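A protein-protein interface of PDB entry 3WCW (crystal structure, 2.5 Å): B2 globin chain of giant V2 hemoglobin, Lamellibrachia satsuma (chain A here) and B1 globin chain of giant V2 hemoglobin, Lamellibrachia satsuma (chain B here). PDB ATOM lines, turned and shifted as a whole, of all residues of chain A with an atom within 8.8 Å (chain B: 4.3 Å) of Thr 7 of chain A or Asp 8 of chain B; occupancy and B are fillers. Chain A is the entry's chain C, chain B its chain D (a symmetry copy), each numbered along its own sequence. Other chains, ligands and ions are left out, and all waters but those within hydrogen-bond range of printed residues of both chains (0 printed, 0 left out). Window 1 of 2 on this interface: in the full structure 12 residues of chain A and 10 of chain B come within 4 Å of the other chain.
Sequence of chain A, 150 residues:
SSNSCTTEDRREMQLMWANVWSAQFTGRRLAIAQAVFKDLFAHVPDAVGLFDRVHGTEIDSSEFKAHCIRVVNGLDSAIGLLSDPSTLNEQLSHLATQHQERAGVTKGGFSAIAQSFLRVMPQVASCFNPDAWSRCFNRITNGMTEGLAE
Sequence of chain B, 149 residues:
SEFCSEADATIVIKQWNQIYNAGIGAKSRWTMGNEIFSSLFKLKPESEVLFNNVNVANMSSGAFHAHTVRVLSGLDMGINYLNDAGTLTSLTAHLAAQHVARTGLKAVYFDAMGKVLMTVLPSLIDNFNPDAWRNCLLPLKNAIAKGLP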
ATOM      1  N   SER A   2      24.485  -2.247 -29.246  1.00  0.00           N
ATOM      2  CA  SER A   2      25.304  -1.041 -29.145  1.00  0.00           C
ATOM      3  C   SER A   2      26.356  -1.254 -28.055  1.00  0.00           C
ATOM      4  O   SER A   2      26.080  -1.871 -27.021  1.00  0.00           O
ATOM      5  CB  SER A   2      24.421   0.167 -28.806  1.00  0.00           C
ATOM      6  OG  SER A   2      25.171   1.369 -28.794  1.00  0.00           O
ATOM      7  N   ASN A   3      27.563  -0.750 -28.291  1.00  0.00           N
ATOM      8  CA  ASN A   3      28.639  -0.905 -27.323  1.00  0.00           C
ATOM      9  C   ASN A   3      28.763   0.305 -26.416  1.00  0.00           C
ATOM     10  O   ASN A   3      29.685   0.388 -25.595  1.00  0.00           O
ATOM     11  CB  ASN A   3      29.971  -1.135 -28.035  1.00  0.00           C
ATOM     12  CG  ASN A   3      30.556  -2.501 -27.742  1.00  0.00           C
ATOM     13  OD1 ASN A   3      31.763  -2.719 -27.893  1.00  0.00           O
ATOM     14  ND2 ASN A   3      29.701  -3.436 -27.329  1.00  0.00           N
ATOM     15  N   SER A   4      27.829   1.239 -26.562  1.00  0.00           N
ATOM     16  CA  SER A   4      27.846   2.455 -25.766  1.00  0.00           C
ATOM     17  C   SER A   4      27.652   2.240 -24.263  1.00  0.00           C
ATOM     18  O   SER A   4      26.831   1.423 -23.839  1.00  0.00           O
ATOM     19  CB  SER A   4      26.782   3.425 -26.285  1.00  0.00           C
ATOM     20  OG  SER A   4      27.263   4.171 -27.393  1.00  0.00           O
ATOM     21  N   CYS A   5      28.426   2.972 -23.463  1.00  0.00           N
ATOM     22  CA  CYS A   5      28.306   2.898 -22.015  1.00  0.00           C
ATOM     23  C   CYS A   5      27.068   3.734 -21.682  1.00  0.00           C
ATOM     24  O   CYS A   5      27.099   4.962 -21.732  1.00  0.00           O
ATOM     25  CB  CYS A   5      29.565   3.464 -21.333  1.00  0.00           C
ATOM     26  SG  CYS A   5      29.409   3.838 -19.550  1.00  0.00           S
ATOM     27  N   THR A   6      25.975   3.046 -21.364  1.00  0.00           N
ATOM     28  CA  THR A   6      24.706   3.690 -21.053  1.00  0.00           C
ATOM     29  C   THR A   6      24.625   4.228 -19.634  1.00  0.00           C
ATOM     30  O   THR A   6      25.497   3.978 -18.795  1.00  0.00           O
ATOM     31  CB  THR A   6      23.542   2.716 -21.247  1.00  0.00           C
ATOM     32  OG1 THR A   6      23.571   1.730 -20.210  1.00  0.00           O
ATOM     33  CG2 THR A   6      23.656   2.012 -22.593  1.00  0.00           C
ATOM     34  N   THR A   7      23.565   4.978 -19.370  1.00  0.00           N
ATOM     35  CA  THR A   7      23.374   5.531 -18.046  1.00  0.00           C
ATOM     36  C   THR A   7      23.215   4.394 -17.047  1.00  0.00           C
ATOM     37  O   THR A   7      23.704   4.476 -15.922  1.00  0.00           O
ATOM     38  CB  THR A   7      22.130   6.435 -17.985  1.00  0.00           C
ATOM     39  OG1 THR A   7      22.388   7.660 -18.689  1.00  0.00           O
ATOM     40  CG2 THR A   7      21.763   6.722 -16.539  1.00  0.00           C
ATOM     41  N   GLU A   8      22.532   3.332 -17.457  1.00  0.00           N
ATOM     42  CA  GLU A   8      22.330   2.191 -16.574  1.00  0.00           C
ATOM     43  C   GLU A   8      23.635   1.449 -16.342  1.00  0.00           C
ATOM     44  O   GLU A   8      23.903   0.977 -15.240  1.00  0.00           O
ATOM     45  CB  GLU A   8      21.262   1.233 -17.132  1.00  0.00           C
ATOM     46  CG  GLU A   8      20.998   1.336 -18.624  1.00  0.00           C
ATOM     47  CD  GLU A   8      19.953   2.387 -18.983  1.00  0.00           C
ATOM     48  OE1 GLU A   8      18.761   2.222 -18.629  1.00  0.00           O
ATOM     49  OE2 GLU A   8      20.333   3.381 -19.629  1.00  0.00           O
ATOM     50  N   ASP A   9      24.457   1.349 -17.375  1.00  0.00           N
ATOM     51  CA  ASP A   9      25.738   0.674 -17.227  1.00  0.00           C
ATOM     52  C   ASP A   9      26.644   1.439 -16.272  1.00  0.00           C
ATOM     53  O   ASP A   9      27.394   0.842 -15.518  1.00  0.00           O
ATOM     54  CB  ASP A   9      26.416   0.521 -18.580  1.00  0.00           C
ATOM     55  CG  ASP A   9      25.708  -0.481 -19.467  1.00  0.00           C
ATOM     56  OD1 ASP A   9      25.034  -1.382 -18.907  1.00  0.00           O
ATOM     57  OD2 ASP A   9      25.839  -0.375 -20.714  1.00  0.00           O
ATOM     58  N   ARG A  10      26.563   2.763 -16.294  1.00  0.00           N
ATOM     59  CA  ARG A  10      27.375   3.590 -15.411  1.00  0.00           C
ATOM     60  C   ARG A  10      26.996   3.363 -13.957  1.00  0.00           C
ATOM     61  O   ARG A  10      27.865   3.271 -13.087  1.00  0.00           O
ATOM     62  CB  ARG A  10      27.210   5.056 -15.792  1.00  0.00           C
ATOM     63  CG  ARG A  10      27.664   5.262 -17.203  1.00  0.00           C
ATOM     64  CD  ARG A  10      27.559   6.665 -17.747  1.00  0.00           C
ATOM     65  NE  ARG A  10      28.115   6.597 -19.094  1.00  0.00           N
ATOM     66  CZ  ARG A  10      28.628   7.612 -19.777  1.00  0.00           C
ATOM     67  NH1 ARG A  10      28.666   8.833 -19.255  1.00  0.00           N
ATOM     68  NH2 ARG A  10      29.137   7.374 -20.983  1.00  0.00           N
ATOM     69  N   ARG A  11      25.699   3.280 -13.686  1.00  0.00           N
ATOM     70  CA  ARG A  11      25.258   3.022 -12.326  1.00  0.00           C
ATOM     71  C   ARG A  11      25.786   1.654 -11.890  1.00  0.00           C
ATOM     72  O   ARG A  11      26.271   1.502 -10.765  1.00  0.00           O
ATOM     73  CB  ARG A  11      23.728   3.062 -12.235  1.00  0.00           C
ATOM     74  CG  ARG A  11      23.166   4.485 -12.267  1.00  0.00           C
ATOM     75  CD  ARG A  11      21.733   4.546 -11.749  1.00  0.00           C
ATOM     76  NE  ARG A  11      20.716   4.513 -12.804  1.00  0.00           N
ATOM     77  CZ  ARG A  11      20.254   5.586 -13.449  1.00  0.00           C
ATOM     78  NH1 ARG A  11      19.325   5.451 -14.392  1.00  0.00           N
ATOM     79  NH2 ARG A  11      20.714   6.796 -13.150  1.00  0.00           N
ATOM     80  N   GLU A  12      25.716   0.671 -12.786  1.00  0.00           N
ATOM     81  CA  GLU A  12      26.195  -0.673 -12.479  1.00  0.00           C
ATOM     82  C   GLU A  12      27.694  -0.734 -12.226  1.00  0.00           C
ATOM     83  O   GLU A  12      28.145  -1.427 -11.306  1.00  0.00           O
ATOM     84  CB  GLU A  12      25.858  -1.651 -13.606  1.00  0.00           C
ATOM     85  CG  GLU A  12      24.439  -2.171 -13.565  1.00  0.00           C
ATOM     86  CD  GLU A  12      24.244  -3.386 -14.454  1.00  0.00           C
ATOM     87  OE1 GLU A  12      24.923  -4.409 -14.216  1.00  0.00           O
ATOM     88  OE2 GLU A  12      23.413  -3.319 -15.385  1.00  0.00           O
ATOM     89  N   MET A  13      28.469  -0.038 -13.052  1.00  0.00           N
ATOM     90  CA  MET A  13      29.912  -0.043 -12.877  1.00  0.00           C
ATOM     91  C   MET A  13      30.272   0.554 -11.529  1.00  0.00           C
ATOM     92  O   MET A  13      31.098  -0.005 -10.806  1.00  0.00           O
ATOM     93  CB  MET A  13      30.615   0.742 -13.987  1.00  0.00           C
ATOM     94  CG  MET A  13      32.122   0.794 -13.806  1.00  0.00           C
ATOM     95  SD  MET A  13      33.027   1.349 -15.257  1.00  0.00           S
ATOM     96  CE  MET A  13      34.643   0.537 -15.020  1.00  0.00           C
ATOM     97  N   GLN A  14      29.653   1.682 -11.188  1.00  0.00           N
ATOM     98  CA  GLN A  14      29.925   2.325  -9.917  1.00  0.00           C
ATOM     99  C   GLN A  14      29.572   1.403  -8.757  1.00  0.00           C
ATOM    100  O   GLN A  14      30.264   1.405  -7.737  1.00  0.00           O
ATOM    101  CB  GLN A  14      29.157   3.641  -9.804  1.00  0.00           C
ATOM    102  CG  GLN A  14      29.737   4.747 -10.661  1.00  0.00           C
ATOM    103  CD  GLN A  14      28.783   5.916 -10.843  1.00  0.00           C
ATOM    104  OE1 GLN A  14      29.157   6.953 -11.386  1.00  0.00           O
ATOM    105  NE2 GLN A  14      27.547   5.750 -10.401  1.00  0.00           N
ATOM    106  N   LEU A  82      31.682   9.192 -14.451  1.00  0.00           N
ATOM    107  CA  LEU A  82      30.811   8.702 -15.519  1.00  0.00           C
ATOM    108  C   LEU A  82      29.444   9.403 -15.404  1.00  0.00           C
ATOM    109  O   LEU A  82      28.696   9.479 -16.373  1.00  0.00           O
ATOM    110  CB  LEU A  82      30.652   7.182 -15.419  1.00  0.00           C
ATOM    111  CG  LEU A  82      31.897   6.393 -15.839  1.00  0.00           C
ATOM    112  CD1 LEU A  82      31.779   4.947 -15.437  1.00  0.00           C
ATOM    113  CD2 LEU A  82      32.077   6.507 -17.356  1.00  0.00           C
ATOM    114  N   SER A  83      29.144   9.926 -14.213  1.00  0.00           N
ATOM    115  CA  SER A  83      27.897  10.639 -13.942  1.00  0.00           C
ATOM    116  C   SER A  83      27.908  12.075 -14.438  1.00  0.00           C
ATOM    117  O   SER A  83      26.868  12.725 -14.457  1.00  0.00           O
ATOM    118  CB  SER A  83      27.610  10.675 -12.443  1.00  0.00           C
ATOM    119  OG  SER A  83      27.364   9.385 -11.935  1.00  0.00           O
ATOM    120  N   PRO A  85      29.842  13.442 -17.608  1.00  0.00           N
ATOM    121  CA  PRO A  85      30.660  13.342 -18.820  1.00  0.00           C
ATOM    122  C   PRO A  85      31.445  14.590 -19.226  1.00  0.00           C
ATOM    123  O   PRO A  85      32.532  14.472 -19.799  1.00  0.00           O
ATOM    124  CB  PRO A  85      29.646  12.917 -19.876  1.00  0.00           C
ATOM    125  CG  PRO A  85      28.692  12.097 -19.092  1.00  0.00           C
ATOM    126  CD  PRO A  85      28.479  12.953 -17.879  1.00  0.00           C
ATOM    127  N   ARG A 135      31.717  -2.352 -21.131  1.00  0.00           N
ATOM    128  CA  ARG A 135      31.339  -1.232 -21.988  1.00  0.00           C
ATOM    129  C   ARG A 135      31.836   0.109 -21.461  1.00  0.00           C
ATOM    130  O   ARG A 135      32.396   0.911 -22.210  1.00  0.00           O
ATOM    131  CB  ARG A 135      29.823  -1.198 -22.210  1.00  0.00           C
ATOM    132  CG  ARG A 135      29.317  -2.308 -23.143  1.00  0.00           C
ATOM    133  CD  ARG A 135      27.865  -2.108 -23.569  1.00  0.00           C
ATOM    134  NE  ARG A 135      26.935  -2.306 -22.458  1.00  0.00           N
ATOM    135  CZ  ARG A 135      26.478  -3.491 -22.066  1.00  0.00           C
ATOM    136  NH1 ARG A 135      25.640  -3.578 -21.045  1.00  0.00           N
ATOM    137  NH2 ARG A 135      26.843  -4.589 -22.711  1.00  0.00           N
ATOM    138  N   CYS A 136      31.663   0.347 -20.168  1.00  0.00           N
ATOM    139  CA  CYS A 136      32.099   1.610 -19.589  1.00  0.00           C
ATOM    140  C   CYS A 136      33.619   1.710 -19.387  1.00  0.00           C
ATOM    141  O   CYS A 136      34.181   2.810 -19.380  1.00  0.00           O
ATOM    142  CB  CYS A 136      31.336   1.862 -18.282  1.00  0.00           C
ATOM    143  SG  CYS A 136      29.542   2.049 -18.583  1.00  0.00           S
ATOM    144  N   SER B   5      19.361   3.869 -24.951  1.00  0.00           N
ATOM    145  CA  SER B   5      18.596   3.370 -23.801  1.00  0.00           C
ATOM    146  C   SER B   5      17.527   4.281 -23.178  1.00  0.00           C
ATOM    147  O   SER B   5      17.530   5.504 -23.332  1.00  0.00           O
ATOM    148  CB  SER B   5      19.568   2.929 -22.704  1.00  0.00           C
ATOM    149  OG  SER B   5      20.275   4.040 -22.174  1.00  0.00           O
ATOM    150  N   GLU B   6      16.607   3.660 -22.453  1.00  0.00           N
ATOM    151  CA  GLU B   6      15.548   4.404 -21.801  1.00  0.00           C
ATOM    152  C   GLU B   6      16.134   5.480 -20.870  1.00  0.00           C
ATOM    153  O   GLU B   6      15.666   6.617 -20.857  1.00  0.00           O
ATOM    154  CB  GLU B   6      14.639   3.441 -21.028  1.00  0.00           C
ATOM    155  CG  GLU B   6      13.567   4.117 -20.171  1.00  0.00           C
ATOM    156  CD  GLU B   6      12.662   3.105 -19.467  1.00  0.00           C
ATOM    157  OE1 GLU B   6      11.883   2.421 -20.173  1.00  0.00           O
ATOM    158  OE2 GLU B   6      12.733   2.986 -18.216  1.00  0.00           O
ATOM    159  N   ALA B   7      17.160   5.125 -20.103  1.00  0.00           N
ATOM    160  CA  ALA B   7      17.797   6.079 -19.188  1.00  0.00           C
ATOM    161  C   ALA B   7      18.515   7.189 -19.955  1.00  0.00           C
ATOM    162  O   ALA B   7      18.422   8.362 -19.587  1.00  0.00           O
ATOM    163  CB  ALA B   7      18.787   5.357 -18.274  1.00  0.00           C
ATOM    164  N   ASP B   8      19.235   6.813 -21.013  1.00  0.00           N
ATOM    165  CA  ASP B   8      19.961   7.789 -21.832  1.00  0.00           C
ATOM    166  C   ASP B   8      19.004   8.779 -22.479  1.00  0.00           C
ATOM    167  O   ASP B   8      19.257   9.982 -22.476  1.00  0.00           O
ATOM    168  CB  ASP B   8      20.765   7.092 -22.946  1.00  0.00           C
ATOM    169  CG  ASP B   8      22.112   6.577 -22.472  1.00  0.00           C
ATOM    170  OD1 ASP B   8      22.767   5.844 -23.251  1.00  0.00           O
ATOM    171  OD2 ASP B   8      22.520   6.909 -21.332  1.00  0.00           O
ATOM    172  N   ALA B   9      17.914   8.253 -23.036  1.00  0.00           N
ATOM    173  CA  ALA B   9      16.892   9.055 -23.705  1.00  0.00           C
ATOM    174  C   ALA B   9      16.219   9.965 -22.692  1.00  0.00           C
ATOM    175  O   ALA B   9      16.018  11.149 -22.944  1.00  0.00           O
ATOM    176  CB  ALA B   9      15.867   8.140 -24.366  1.00  0.00           C
ATOM    177  N   THR B  10      15.874   9.405 -21.541  1.00  0.00           N
ATOM    178  CA  THR B  10      15.256  10.182 -20.481  1.00  0.00           C
ATOM    179  C   THR B  10      16.053  11.463 -20.251  1.00  0.00           C
ATOM    180  O   THR B  10      15.494  12.554 -20.154  1.00  0.00           O
ATOM    181  CB  THR B  10      15.245   9.402 -19.170  1.00  0.00           C
ATOM    182  OG1 THR B  10      14.410   8.251 -19.315  1.00  0.00           O
ATOM    183  CG2 THR B  10      14.739  10.282 -18.027  1.00  0.00           C
ATOM    184  N   ILE B  11      17.370  11.324 -20.168  1.00  0.00           N
ATOM    185  CA  ILE B  11      18.213  12.483 -19.940  1.00  0.00           C
ATOM    186  C   ILE B  11      18.143  13.462 -21.090  1.00  0.00           C
ATOM    187  O   ILE B  11      17.917  14.656 -20.869  1.00  0.00           O
ATOM    188  CB  ILE B  11      19.679  12.084 -19.703  1.00  0.00           C
ATOM    189  CG1 ILE B  11      19.789  11.293 -18.398  1.00  0.00           C
ATOM    190  CG2 ILE B  11      20.538  13.333 -19.627  1.00  0.00           C
ATOM    191  CD1 ILE B  11      21.198  10.902 -18.039  1.00  0.00           C
ATOM    192  N   VAL B  12      18.322  12.965 -22.314  1.00  0.00           N
ATOM    193  CA  VAL B  12      18.279  13.831 -23.488  1.00  0.00           C
ATOM    194  C   VAL B  12      16.951  14.593 -23.577  1.00  0.00           C
ATOM    195  O   VAL B  12      16.927  15.819 -23.657  1.00  0.00           O
ATOM    196  CB  VAL B  12      18.488  13.017 -24.778  1.00  0.00           C
ATOM    197  CG1 VAL B  12      18.377  13.930 -26.003  1.00  0.00           C
ATOM    198  CG2 VAL B  12      19.849  12.356 -24.742  1.00  0.00           C
ATOM    199  N   ALA B 132      25.258  11.041 -23.047  1.00  0.00           N
ATOM    200  CA  ALA B 132      23.902  10.574 -23.283  1.00  0.00           C
ATOM    201  C   ALA B 132      23.421  11.105 -24.631  1.00  0.00           C
ATOM    202  O   ALA B 132      22.659  10.436 -25.333  1.00  0.00           O
ATOM    203  CB  ALA B 132      22.972  11.046 -22.161  1.00  0.00           C
ATOM    204  N   ASN B 135      25.117   9.175 -27.431  1.00  0.00           N
ATOM    205  CA  ASN B 135      24.469   7.871 -27.529  1.00  0.00           C
ATOM    206  C   ASN B 135      23.143   7.928 -28.275  1.00  0.00           C
ATOM    207  O   ASN B 135      22.796   7.002 -29.007  1.00  0.00           O
ATOM    208  CB  ASN B 135      24.224   7.273 -26.139  1.00  0.00           C
ATOM    209  CG  ASN B 135      25.506   6.853 -25.450  1.00  0.00           C
ATOM    210  OD1 ASN B 135      26.557   6.709 -26.090  1.00  0.00           O
ATOM    211  ND2 ASN B 135      25.422   6.630 -24.140  1.00  0.00           N
ATOM    212  N   CYS B 136      22.394   9.010 -28.092  1.00  0.00           N
ATOM    213  CA  CYS B 136      21.107   9.122 -28.753  1.00  0.00           C
ATOM    214  C   CYS B 136      21.161   9.845 -30.088  1.00  0.00           C
ATOM    215  O   CYS B 136      20.543   9.408 -31.041  1.00  0.00           O
ATOM    216  CB  CYS B 136      20.100   9.810 -27.836  1.00  0.00           C
ATOM    217  SG  CYS B 136      19.751   8.900 -26.303  1.00  0.00           S
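Printed residues of chain B within 4 Å of Ser 4 of chain A: Asn 135.
Printed residues of chain B within 4 Å of Cys 5 of chain A: Asn 135 (3.4 Å).
Of the printed residues of chain B, Thr 6 of chain A touches Ser 5 and Asp 8.
Glu 6 of chain B touches none of the printed residues of chain A.
Ala 7 of chain B touches three residues of chain A.
Of chain A, only Thr 6 (3.6 Å), Thr 7 (2.8 Å) and Glu 8 (3.9 Å) come within 4 Å of Asp 8 of chain B.
Printed residues of chain A within 4 Å of Ile 11 of chain B: Thr 7.
Printed residues of chain A within 4 Å of Asn 135 of chain B: Ser 4 and Cys 5.
The nearest residue of chain A that does not touch Asp 8 of chain B is Cys 5 of chain A (4.7 Å).
Printed residues of chain B that touch a printed residue of chain A: Ser 5, Ala 7, Asp 8, Ile 11 and Asn 135.
Among the printed residues, 11 pairs touch across the chains.
Among the printed residues, no Asp or Glu carboxylate lies within 4 Å of a Lys or Arg side-chain nitrogen of the other chain.
Among the printed residues, merely in contact across the chains: Thr 6 of chain A with Ser 5 of chain B, Thr 6 of chain A with Asp 8 of chain B, Thr 7 of chain A with Ala 7 of chain B, Thr 7 of chain A with Ile 11 of chain B, Glu 8 of chain A with Ala 7 of chain B, Glu 8 of chain A with Asp 8 of chain B and Arg 11 of chain A with Ala 7 of chain B.
The side-chain amide nitrogen of Asn 135 of chain B sits at hydrogen-bond distance from the side-chain carboxylate of Asp 8 of chain B (2.9 Å).
The side-chain sulfur of Cys 5 of chain A sits at hydrogen-bond distance from the guanidinium group of Arg 10 of chain A (3.1 Å).
N of Asp 8 of chain B lies close to OG of Ser 5 of chain B (3.2 Å).
OG1 of Thr 6 of chain A sits close to N of Glu 8 of chain A (3.4 Å).
The side-chain hydroxyl (OG1) of Thr 6 of chain A lies within hydrogen-bond range of the backbone NH (N) of Asp 9 of chain A (3.0 Å).
The side-chain sulfur (SG) of Cys 5 of chain A forms a disulfide with the side-chain sulfur (SG) of Cys 136 of chain A (2.0 Å).
OD1 of Asn 135 of chain B is in hydrogen-bond range of OG of Ser 4 of chain A.
The backbone carbonyl oxygen (O) of Cys 5 of chain A lies within hydrogen-bond range of the side-chain amide nitrogen (ND2) of Asn 135 of chain B (3.4 Å).
The side-chain carboxylate (OE2) of Glu 8 of chain A sits at hydrogen-bond distance from the side-chain hydroxyl (OG) of Ser 5 of chain B, 2.6 Å away.
OD2 of Asp 8 of chain B lies within hydrogen-bond range of OG1 of Thr 7 of chain A (2.8 Å).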
